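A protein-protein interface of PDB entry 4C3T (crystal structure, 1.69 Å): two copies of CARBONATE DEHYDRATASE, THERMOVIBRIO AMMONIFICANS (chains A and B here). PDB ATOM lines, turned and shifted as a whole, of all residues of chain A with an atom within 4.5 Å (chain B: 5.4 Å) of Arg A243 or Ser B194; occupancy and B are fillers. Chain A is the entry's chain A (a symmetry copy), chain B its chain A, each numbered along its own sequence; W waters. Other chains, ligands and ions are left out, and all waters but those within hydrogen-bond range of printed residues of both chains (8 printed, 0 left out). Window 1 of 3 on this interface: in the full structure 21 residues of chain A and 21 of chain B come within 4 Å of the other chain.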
ATOM      1  N   LYS A  51      22.545 -18.437  -9.184  1.00  0.00           N
ATOM      2  CA  LYS A  51      23.750 -19.012  -9.760  1.00  0.00           C
ATOM      3  C   LYS A  51      23.941 -20.489  -9.432  1.00  0.00           C
ATOM      4  O   LYS A  51      24.956 -21.066  -9.808  1.00  0.00           O
ATOM      5  CB  LYS A  51      24.999 -18.234  -9.306  1.00  0.00           C
ATOM      6  CG  LYS A  51      24.971 -16.745  -9.617  1.00  0.00           C
ATOM      7  CD  LYS A  51      25.035 -16.516 -11.118  1.00  0.00           C
ATOM      8  CE  LYS A  51      24.889 -15.049 -11.468  1.00  0.00           C
ATOM      9  NZ  LYS A  51      24.736 -14.861 -12.937  1.00  0.00           N
ATOM     10  N   ASN A  52      22.978 -21.072  -8.709  1.00  0.00           N
ATOM     11  CA  ASN A  52      23.027 -22.469  -8.274  1.00  0.00           C
ATOM     12  C   ASN A  52      21.727 -23.175  -8.622  1.00  0.00           C
ATOM     13  O   ASN A  52      21.073 -23.828  -7.802  1.00  0.00           O
ATOM     14  CB  ASN A  52      23.384 -22.569  -6.751  1.00  0.00           C
ATOM     15  CG  ASN A  52      24.775 -22.031  -6.444  1.00  0.00           C
ATOM     16  OD1 ASN A  52      25.767 -22.746  -6.524  1.00  0.00           O
ATOM     17  ND2 ASN A  52      24.846 -20.755  -6.090  1.00  0.00           N
ATOM     18  N   GLN A  53      21.377 -23.093  -9.915  1.00  0.00           N
ATOM     19  CA  GLN A  53      20.093 -23.568 -10.406  1.00  0.00           C
ATOM     20  C   GLN A  53      20.132 -25.022 -10.947  1.00  0.00           C
ATOM     21  O   GLN A  53      21.195 -25.555 -11.244  1.00  0.00           O
ATOM     22  CB  GLN A  53      19.586 -22.609 -11.500  1.00  0.00           C
ATOM     23  CG  GLN A  53      19.117 -21.239 -11.000  1.00  0.00           C
ATOM     24  CD  GLN A  53      17.769 -21.304 -10.314  1.00  0.00           C
ATOM     25  OE1 GLN A  53      16.715 -21.473 -10.952  1.00  0.00           O
ATOM     26  NE2 GLN A  53      17.782 -21.143  -8.985  1.00  0.00           N
ATOM     27  N   ILE A  56      20.972 -29.636 -14.368  1.00  0.00           N
ATOM     28  CA  ILE A  56      22.268 -29.435 -14.962  1.00  0.00           C
ATOM     29  C   ILE A  56      22.627 -30.602 -15.862  1.00  0.00           C
ATOM     30  O   ILE A  56      21.979 -31.657 -15.810  1.00  0.00           O
ATOM     31  CB  ILE A  56      23.388 -29.268 -13.891  1.00  0.00           C
ATOM     32  CG1 ILE A  56      23.440 -30.483 -12.941  1.00  0.00           C
ATOM     33  CG2 ILE A  56      23.181 -27.968 -13.131  1.00  0.00           C
ATOM     34  CD1 ILE A  56      24.743 -30.560 -12.172  1.00  0.00           C
ATOM     35  N   TYR A 193      24.782 -32.710  -5.956  1.00  0.00           N
ATOM     36  CA  TYR A 193      25.148 -31.298  -6.070  1.00  0.00           C
ATOM     37  C   TYR A 193      24.122 -30.431  -5.348  1.00  0.00           C
ATOM     38  O   TYR A 193      23.032 -30.913  -4.945  1.00  0.00           O
ATOM     39  CB  TYR A 193      25.358 -30.873  -7.560  1.00  0.00           C
ATOM     40  CG  TYR A 193      24.044 -30.701  -8.322  1.00  0.00           C
ATOM     41  CD1 TYR A 193      23.357 -31.801  -8.827  1.00  0.00           C
ATOM     42  CD2 TYR A 193      23.529 -29.425  -8.573  1.00  0.00           C
ATOM     43  CE1 TYR A 193      22.163 -31.633  -9.515  1.00  0.00           C
ATOM     44  CE2 TYR A 193      22.317 -29.237  -9.246  1.00  0.00           C
ATOM     45  CZ  TYR A 193      21.649 -30.359  -9.747  1.00  0.00           C
ATOM     46  OH  TYR A 193      20.440 -30.256 -10.426  1.00  0.00           O
ATOM     47  N   SER A 194      24.492 -29.175  -5.140  1.00  0.00           N
ATOM     48  CA  SER A 194      23.637 -28.199  -4.504  1.00  0.00           C
ATOM     49  C   SER A 194      22.962 -27.412  -5.612  1.00  0.00           C
ATOM     50  O   SER A 194      23.644 -26.775  -6.420  1.00  0.00           O
ATOM     51  CB  SER A 194      24.509 -27.232  -3.707  1.00  0.00           C
ATOM     52  OG  SER A 194      23.753 -26.132  -3.194  1.00  0.00           O
ATOM     53  N   GLY A 195      21.652 -27.467  -5.661  1.00  0.00           N
ATOM     54  CA  GLY A 195      20.932 -26.747  -6.705  1.00  0.00           C
ATOM     55  C   GLY A 195      19.618 -26.145  -6.251  1.00  0.00           C
ATOM     56  O   GLY A 195      19.528 -25.476  -5.221  1.00  0.00           O
ATOM     57  N   PRO A 239      23.599 -23.317 -16.022  1.00  0.00           N
ATOM     58  CA  PRO A 239      25.061 -23.305 -15.895  1.00  0.00           C
ATOM     59  C   PRO A 239      25.511 -23.810 -14.527  1.00  0.00           C
ATOM     60  O   PRO A 239      24.891 -23.460 -13.491  1.00  0.00           O
ATOM     61  CB  PRO A 239      25.436 -21.824 -16.037  1.00  0.00           C
ATOM     62  CG  PRO A 239      24.238 -21.163 -16.631  1.00  0.00           C
ATOM     63  CD  PRO A 239      23.041 -21.974 -16.251  1.00  0.00           C
ATOM     64  N   LEU A 240      26.561 -24.612 -14.536  1.00  0.00           N
ATOM     65  CA  LEU A 240      27.139 -25.152 -13.309  1.00  0.00           C
ATOM     66  C   LEU A 240      27.736 -24.042 -12.439  1.00  0.00           C
ATOM     67  O   LEU A 240      27.688 -24.117 -11.188  1.00  0.00           O
ATOM     68  CB  LEU A 240      28.205 -26.184 -13.657  1.00  0.00           C
ATOM     69  CG  LEU A 240      28.792 -27.025 -12.529  1.00  0.00           C
ATOM     70  CD1 LEU A 240      27.830 -28.104 -12.042  1.00  0.00           C
ATOM     71  CD2 LEU A 240      30.102 -27.623 -13.000  1.00  0.00           C
ATOM     72  N   ASN A 241      28.282 -23.015 -13.096  1.00  0.00           N
ATOM     73  CA  ASN A 241      28.941 -21.899 -12.417  1.00  0.00           C
ATOM     74  C   ASN A 241      30.055 -22.407 -11.496  1.00  0.00           C
ATOM     75  O   ASN A 241      30.983 -23.066 -11.962  1.00  0.00           O
ATOM     76  CB  ASN A 241      27.904 -20.978 -11.746  1.00  0.00           C
ATOM     77  CG  ASN A 241      26.980 -20.329 -12.770  1.00  0.00           C
ATOM     78  OD1 ASN A 241      27.440 -19.846 -13.803  1.00  0.00           O
ATOM     79  ND2 ASN A 241      25.684 -20.313 -12.493  1.00  0.00           N
ATOM     80  N   ALA A 242      29.986 -22.104 -10.197  1.00  0.00           N
ATOM     81  CA  ALA A 242      31.082 -22.448  -9.304  1.00  0.00           C
ATOM     82  C   ALA A 242      31.075 -23.896  -8.804  1.00  0.00           C
ATOM     83  O   ALA A 242      32.046 -24.359  -8.189  1.00  0.00           O
ATOM     84  CB  ALA A 242      31.071 -21.478  -8.124  1.00  0.00           C
ATOM     85  N   ARG A 243      30.000 -24.619  -9.084  1.00  0.00           N
ATOM     86  CA  ARG A 243      29.787 -25.955  -8.517  1.00  0.00           C
ATOM     87  C   ARG A 243      30.558 -27.089  -9.149  1.00  0.00           C
ATOM     88  O   ARG A 243      30.916 -27.040 -10.331  1.00  0.00           O
ATOM     89  CB  ARG A 243      28.322 -26.327  -8.585  1.00  0.00           C
ATOM     90  CG  ARG A 243      27.408 -25.345  -7.866  1.00  0.00           C
ATOM     91  CD  ARG A 243      25.958 -25.685  -8.139  1.00  0.00           C
ATOM     92  NE  ARG A 243      25.573 -25.235  -9.512  1.00  0.00           N
ATOM     93  CZ  ARG A 243      24.341 -25.327  -9.978  1.00  0.00           C
ATOM     94  NH1 ARG A 243      23.371 -25.864  -9.211  1.00  0.00           N
ATOM     95  NH2 ARG A 243      24.064 -24.902 -11.234  1.00  0.00           N
ATOM     96  N   LYS A 244      30.813 -28.100  -8.328  1.00  0.00           N
ATOM     97  CA  LYS A 244      31.222 -29.426  -8.784  1.00  0.00           C
ATOM     98  C   LYS A 244      30.076 -30.391  -8.537  1.00  0.00           C
ATOM     99  O   LYS A 244      29.335 -30.264  -7.535  1.00  0.00           O
ATOM    100  CB  LYS A 244      32.455 -29.929  -8.015  1.00  0.00           C
ATOM    101  CG  LYS A 244      33.805 -29.542  -8.601  1.00  0.00           C
ATOM    102  CD  LYS A 244      33.993 -30.135  -9.992  1.00  0.00           C
ATOM    103  CE  LYS A 244      35.419 -30.018 -10.484  1.00  0.00           C
ATOM    104  NZ  LYS A 244      35.524 -30.532 -11.876  1.00  0.00           N
ATOM    105  N   VAL A 245      29.898 -31.352  -9.440  1.00  0.00           N
ATOM    106  CA  VAL A 245      29.030 -32.472  -9.169  1.00  0.00           C
ATOM    107  C   VAL A 245      29.888 -33.575  -8.531  1.00  0.00           C
ATOM    108  O   VAL A 245      30.950 -33.933  -9.036  1.00  0.00           O
ATOM    109  CB  VAL A 245      28.362 -33.016 -10.461  1.00  0.00           C
ATOM    110  CG1 VAL A 245      27.478 -34.209 -10.146  1.00  0.00           C
ATOM    111  CG2 VAL A 245      27.590 -31.903 -11.160  1.00  0.00           C
ATOM    112  N   ASN B  52      23.776 -19.778  -0.764  1.00  0.00           N
ATOM    113  CA  ASN B  52      25.127 -20.274  -1.032  1.00  0.00           C
ATOM    114  C   ASN B  52      26.154 -19.200  -0.716  1.00  0.00           C
ATOM    115  O   ASN B  52      27.038 -18.857  -1.508  1.00  0.00           O
ATOM    116  CB  ASN B  52      25.245 -20.816  -2.498  1.00  0.00           C
ATOM    117  CG  ASN B  52      24.347 -22.021  -2.746  1.00  0.00           C
ATOM    118  OD1 ASN B  52      24.727 -23.160  -2.501  1.00  0.00           O
ATOM    119  ND2 ASN B  52      23.142 -21.763  -3.235  1.00  0.00           N
ATOM    120  N   SER B  54      29.107 -16.990   1.698  1.00  0.00           N
ATOM    121  CA  SER B  54      30.408 -17.145   2.332  1.00  0.00           C
ATOM    122  C   SER B  54      30.606 -16.050   3.366  1.00  0.00           C
ATOM    123  O   SER B  54      30.033 -14.992   3.276  1.00  0.00           O
ATOM    124  CB  SER B  54      31.505 -17.015   1.292  1.00  0.00           C
ATOM    125  OG  SER B  54      31.353 -18.097   0.378  1.00  0.00           O
ATOM    126  N   ASP B 102      39.637 -25.599 -12.752  1.00  0.00           N
ATOM    127  CA  ASP B 102      38.634 -26.156 -13.676  1.00  0.00           C
ATOM    128  C   ASP B 102      39.120 -25.985 -15.116  1.00  0.00           C
ATOM    129  O   ASP B 102      38.331 -25.685 -16.028  1.00  0.00           O
ATOM    130  CB  ASP B 102      37.241 -25.542 -13.466  1.00  0.00           C
ATOM    131  CG  ASP B 102      36.658 -25.887 -12.096  1.00  0.00           C
ATOM    132  OD1 ASP B 102      37.226 -26.777 -11.442  1.00  0.00           O
ATOM    133  OD2 ASP B 102      35.634 -25.295 -11.701  1.00  0.00           O
ATOM    134  N   ARG B 192      37.415 -26.950  -0.942  1.00  0.00           N
ATOM    135  CA  ARG B 192      36.692 -26.227  -1.993  1.00  0.00           C
ATOM    136  C   ARG B 192      35.189 -26.273  -1.785  1.00  0.00           C
ATOM    137  O   ARG B 192      34.629 -27.316  -1.379  1.00  0.00           O
ATOM    138  CB  ARG B 192      37.051 -26.782  -3.386  1.00  0.00           C
ATOM    139  CG  ARG B 192      36.074 -26.313  -4.440  1.00  0.00           C
ATOM    140  CD  ARG B 192      36.586 -26.586  -5.845  1.00  0.00           C
ATOM    141  NE  ARG B 192      35.599 -26.058  -6.779  1.00  0.00           N
ATOM    142  CZ  ARG B 192      35.797 -26.015  -8.093  1.00  0.00           C
ATOM    143  NH1 ARG B 192      36.935 -26.474  -8.586  1.00  0.00           N
ATOM    144  NH2 ARG B 192      34.863 -25.526  -8.903  1.00  0.00           N
ATOM    145  N   TYR B 193      34.546 -25.136  -2.012  1.00  0.00           N
ATOM    146  CA  TYR B 193      33.085 -25.068  -2.029  1.00  0.00           C
ATOM    147  C   TYR B 193      32.624 -23.926  -2.929  1.00  0.00           C
ATOM    148  O   TYR B 193      33.440 -23.073  -3.364  1.00  0.00           O
ATOM    149  CB  TYR B 193      32.493 -24.977  -0.584  1.00  0.00           C
ATOM    150  CG  TYR B 193      32.654 -23.590   0.039  1.00  0.00           C
ATOM    151  CD1 TYR B 193      33.861 -23.194   0.607  1.00  0.00           C
ATOM    152  CD2 TYR B 193      31.571 -22.707   0.099  1.00  0.00           C
ATOM    153  CE1 TYR B 193      33.997 -21.931   1.168  1.00  0.00           C
ATOM    154  CE2 TYR B 193      31.694 -21.423   0.642  1.00  0.00           C
ATOM    155  CZ  TYR B 193      32.917 -21.052   1.209  1.00  0.00           C
ATOM    156  OH  TYR B 193      33.121 -19.794   1.768  1.00  0.00           O
ATOM    157  N   SER B 194      31.338 -23.943  -3.246  1.00  0.00           N
ATOM    158  CA  SER B 194      30.715 -22.922  -4.059  1.00  0.00           C
ATOM    159  C   SER B 194      30.074 -21.929  -3.109  1.00  0.00           C
ATOM    160  O   SER B 194      29.197 -22.303  -2.325  1.00  0.00           O
ATOM    161  CB  SER B 194      29.604 -23.566  -4.885  1.00  0.00           C
ATOM    162  OG  SER B 194      28.825 -22.591  -5.582  1.00  0.00           O
ATOM    163  N   GLY B 195      30.509 -20.693  -3.165  1.00  0.00           N
ATOM    164  CA  GLY B 195      29.949 -19.683  -2.274  1.00  0.00           C
ATOM    165  C   GLY B 195      29.804 -18.312  -2.902  1.00  0.00           C
ATOM    166  O   GLY B 195      29.281 -18.152  -4.005  1.00  0.00           O
ATOM    167  N   SER B 196      30.221 -17.297  -2.161  1.00  0.00           N
ATOM    168  CA  SER B 196      29.875 -15.922  -2.516  1.00  0.00           C
ATOM    169  C   SER B 196      31.006 -14.970  -2.144  1.00  0.00           C
ATOM    170  O   SER B 196      31.943 -15.356  -1.445  1.00  0.00           O
ATOM    171  CB  SER B 196      28.588 -15.467  -1.792  1.00  0.00           C
ATOM    172  OG  SER B 196      28.897 -15.088  -0.415  1.00  0.00           O
ATOM    173  N   GLY B 205      27.910 -17.745  -7.174  1.00  0.00           N
ATOM    174  CA  GLY B 205      28.780 -18.351  -8.213  1.00  0.00           C
ATOM    175  C   GLY B 205      30.268 -18.137  -8.042  1.00  0.00           C
ATOM    176  O   GLY B 205      31.016 -18.115  -9.020  1.00  0.00           O
ATOM    177  N   VAL B 206      30.724 -18.001  -6.788  1.00  0.00           N
ATOM    178  CA  VAL B 206      32.138 -17.829  -6.492  1.00  0.00           C
ATOM    179  C   VAL B 206      32.802 -19.172  -6.109  1.00  0.00           C
ATOM    180  O   VAL B 206      32.309 -19.889  -5.231  1.00  0.00           O
ATOM    181  CB  VAL B 206      32.338 -16.765  -5.353  1.00  0.00           C
ATOM    182  CG1 VAL B 206      33.828 -16.669  -5.017  1.00  0.00           C
ATOM    183  CG2 VAL B 206      31.798 -15.404  -5.790  1.00  0.00           C
ATOM    184  N   ARG B 207      33.912 -19.531  -6.774  1.00  0.00           N
ATOM    185  CA  ARG B 207      34.680 -20.713  -6.439  1.00  0.00           C
ATOM    186  C   ARG B 207      35.604 -20.360  -5.272  1.00  0.00           C
ATOM    187  O   ARG B 207      36.398 -19.425  -5.363  1.00  0.00           O
ATOM    188  CB  ARG B 207      35.561 -21.135  -7.622  1.00  0.00           C
ATOM    189  CG  ARG B 207      34.767 -21.707  -8.792  1.00  0.00           C
ATOM    190  CD  ARG B 207      35.647 -21.648 -10.042  1.00  0.00           C
ATOM    191  NE  ARG B 207      35.179 -22.523 -11.137  1.00  0.00           N
ATOM    192  CZ  ARG B 207      34.348 -22.156 -12.116  1.00  0.00           C
ATOM    193  NH1 ARG B 207      33.801 -20.949 -12.141  1.00  0.00           N
ATOM    194  NH2 ARG B 207      34.036 -23.036 -13.078  1.00  0.00           N
ATOM    195  N   TRP B 208      35.466 -21.097  -4.168  1.00  0.00           N
ATOM    196  CA  TRP B 208      36.367 -20.911  -3.034  1.00  0.00           C
ATOM    197  C   TRP B 208      37.388 -22.041  -2.937  1.00  0.00           C
ATOM    198  O   TRP B 208      37.040 -23.236  -2.959  1.00  0.00           O
ATOM    199  CB  TRP B 208      35.567 -20.756  -1.708  1.00  0.00           C
ATOM    200  CG  TRP B 208      35.074 -19.392  -1.489  1.00  0.00           C
ATOM    201  CD1 TRP B 208      33.845 -18.883  -1.828  1.00  0.00           C
ATOM    202  CD2 TRP B 208      35.801 -18.326  -0.902  1.00  0.00           C
ATOM    203  NE1 TRP B 208      33.771 -17.549  -1.481  1.00  0.00           N
ATOM    204  CE2 TRP B 208      34.956 -17.183  -0.901  1.00  0.00           C
ATOM    205  CE3 TRP B 208      37.090 -18.228  -0.358  1.00  0.00           C
ATOM    206  CZ2 TRP B 208      35.361 -15.945  -0.383  1.00  0.00           C
ATOM    207  CZ3 TRP B 208      37.490 -16.988   0.167  1.00  0.00           C
ATOM    208  CH2 TRP B 208      36.622 -15.874   0.154  1.00  0.00           C
ATOM    209  N   ARG B 243      25.039 -27.431   0.603  1.00  0.00           N
ATOM    210  CA  ARG B 243      26.422 -27.675   0.176  1.00  0.00           C
ATOM    211  C   ARG B 243      27.219 -28.660   0.996  1.00  0.00           C
ATOM    212  O   ARG B 243      26.967 -28.853   2.190  1.00  0.00           O
ATOM    213  CB  ARG B 243      27.204 -26.380   0.162  1.00  0.00           C
ATOM    214  CG  ARG B 243      26.600 -25.311  -0.739  1.00  0.00           C
ATOM    215  CD  ARG B 243      27.330 -23.998  -0.552  1.00  0.00           C
ATOM    216  NE  ARG B 243      26.901 -23.347   0.723  1.00  0.00           N
ATOM    217  CZ  ARG B 243      27.314 -22.147   1.092  1.00  0.00           C
ATOM    218  NH1 ARG B 243      28.176 -21.466   0.312  1.00  0.00           N
ATOM    219  NH2 ARG B 243      26.885 -21.619   2.263  1.00  0.00           N
HETATM  220  O   HOH W   1      38.710 -29.321 -11.619  1.00  0.00           O
HETATM  221  O   HOH W   2      32.940 -25.777  -5.864  1.00  0.00           O
HETATM  222  O   HOH W   3      31.582 -24.406 -14.561  1.00  0.00           O
HETATM  223  O   HOH W   4      27.614 -21.516  -8.452  1.00  0.00           O
HETATM  224  O   HOH W   5      27.685 -19.945  -5.316  1.00  0.00           O
HETATM  225  O   HOH W   6      22.847 -24.345  -0.577  1.00  0.00           O
HETATM  226  O   HOH W   7      21.595 -24.321  -3.854  1.00  0.00           O
HETATM  227  O   HOH W   8      26.328 -24.414  -4.383  1.00  0.00           O
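The backbone carbonyl oxygen (O) of Ala A242 sits at hydrogen-bond distance from the guanidinium group (NH2) of Arg B192 (3.1 Å). The side-chain hydroxyl (OG) of Ser A194 sits at hydrogen-bond distance from the side-chain amide oxygen (OD1) of Asn B52 (3.2 Å). The side-chain hydroxyl (OG) of Ser B194 is in hydrogen-bond range of the side-chain amide oxygen (OD1) of Asn A52. ND2 of Asn B52 lies close to ND2 of Asn A52 (3.5 Å). O of Asn A241 sits at hydrogen-bond distance from NH2 of Arg B207.
The guanidinium group (NE) of Arg B207 is in salt-bridge range of the side-chain carboxylate (OD2) of Asp B102. The backbone carbonyl oxygen (O) of Lys A51 sits at hydrogen-bond distance from the side-chain amide nitrogen (ND2) of Asn A241 (2.9 Å). NH1 of Arg A243 sits close to O of Asn A52, 3.4 Å away. The backbone NH (N) of Gly B205 sits at hydrogen-bond distance from the backbone carbonyl oxygen (O) of Gly B195 (3.5 Å). The backbone carbonyl oxygen of Ser B194 lies within hydrogen-bond range of the guanidinium group of Arg B243. The backbone carbonyl oxygen (O) of Leu A240 lies within hydrogen-bond range of the guanidinium group (NE) of Arg A243, at 2.9 Å.
CB of Lys A51 touches N of Gly B205, at 3.6 Å. OG of Ser A194 touches CG of Arg B243 (3.8 Å). Ala A242 touches Ser B194. Ala A242 touches Gly B205 (CB to C, 3.4 Å). Val B206 touches Ala A242. Ala A242 touches Arg B207 (CB to N, 3.7 Å). Arg A243 touches Ser B194. OD1 of Asp B102 touches CE of Lys A244, at 3.8 Å.
Of the printed residues of chain B, Asn A241 touches Arg B207. Arg A243 touches just one residue of chain B: Ser B194. Ser B194 touches just these residues of chain A: Asn A52, Ala A242 and Arg A243. Printed residues of chain A within 4 Å of Val B206: Ala A242 (3.5 Å). Printed residues of chain A within 4 Å of Arg B243: Ser A194. The nearest residue of chain B that does not touch Arg A243 is Arg B192 (4.5 Å).
Hydrophobic or aromatic side chains of chain A that line the printed part of chain B: Ala A242.
Asn B52 touches its own counterpart, Asn A52. Asn A52 touches Ser B194, and with the chains exchanged Ser A194 touches Asn B52. Ser A194 touches Arg B243, and with the chains exchanged Arg A243 touches Ser B194. Of the 13 pairs that touch across the chains among the printed residues, 5 have their exchanged pair printed and touching as well.
Water W7 lies within hydrogen-bond range of O of Gly A195 (2.7 Å), OG of Ser A194 (2.9 Å) and ND2 of Asn B52 (3.1 Å). Water W2 bridges NE of Arg B192 (2.8 Å) and O of Ala A242 (2.9 Å). Water W6 lies within hydrogen-bond range of OD1 of Asn B52 (2.9 Å) and OG of Ser A194 (3.3 Å). Water W4 lies within hydrogen-bond range of OD1 of Asn A52, N of Ala A242, O of Lys A51 and OG of Ser B194. Water W1 lies within hydrogen-bond range of the side-chain carboxylate of Asp B102 and the side-chain amino group of Lys A244. Water W3 bridges O of Asn A241 and NH2 of Arg B207.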
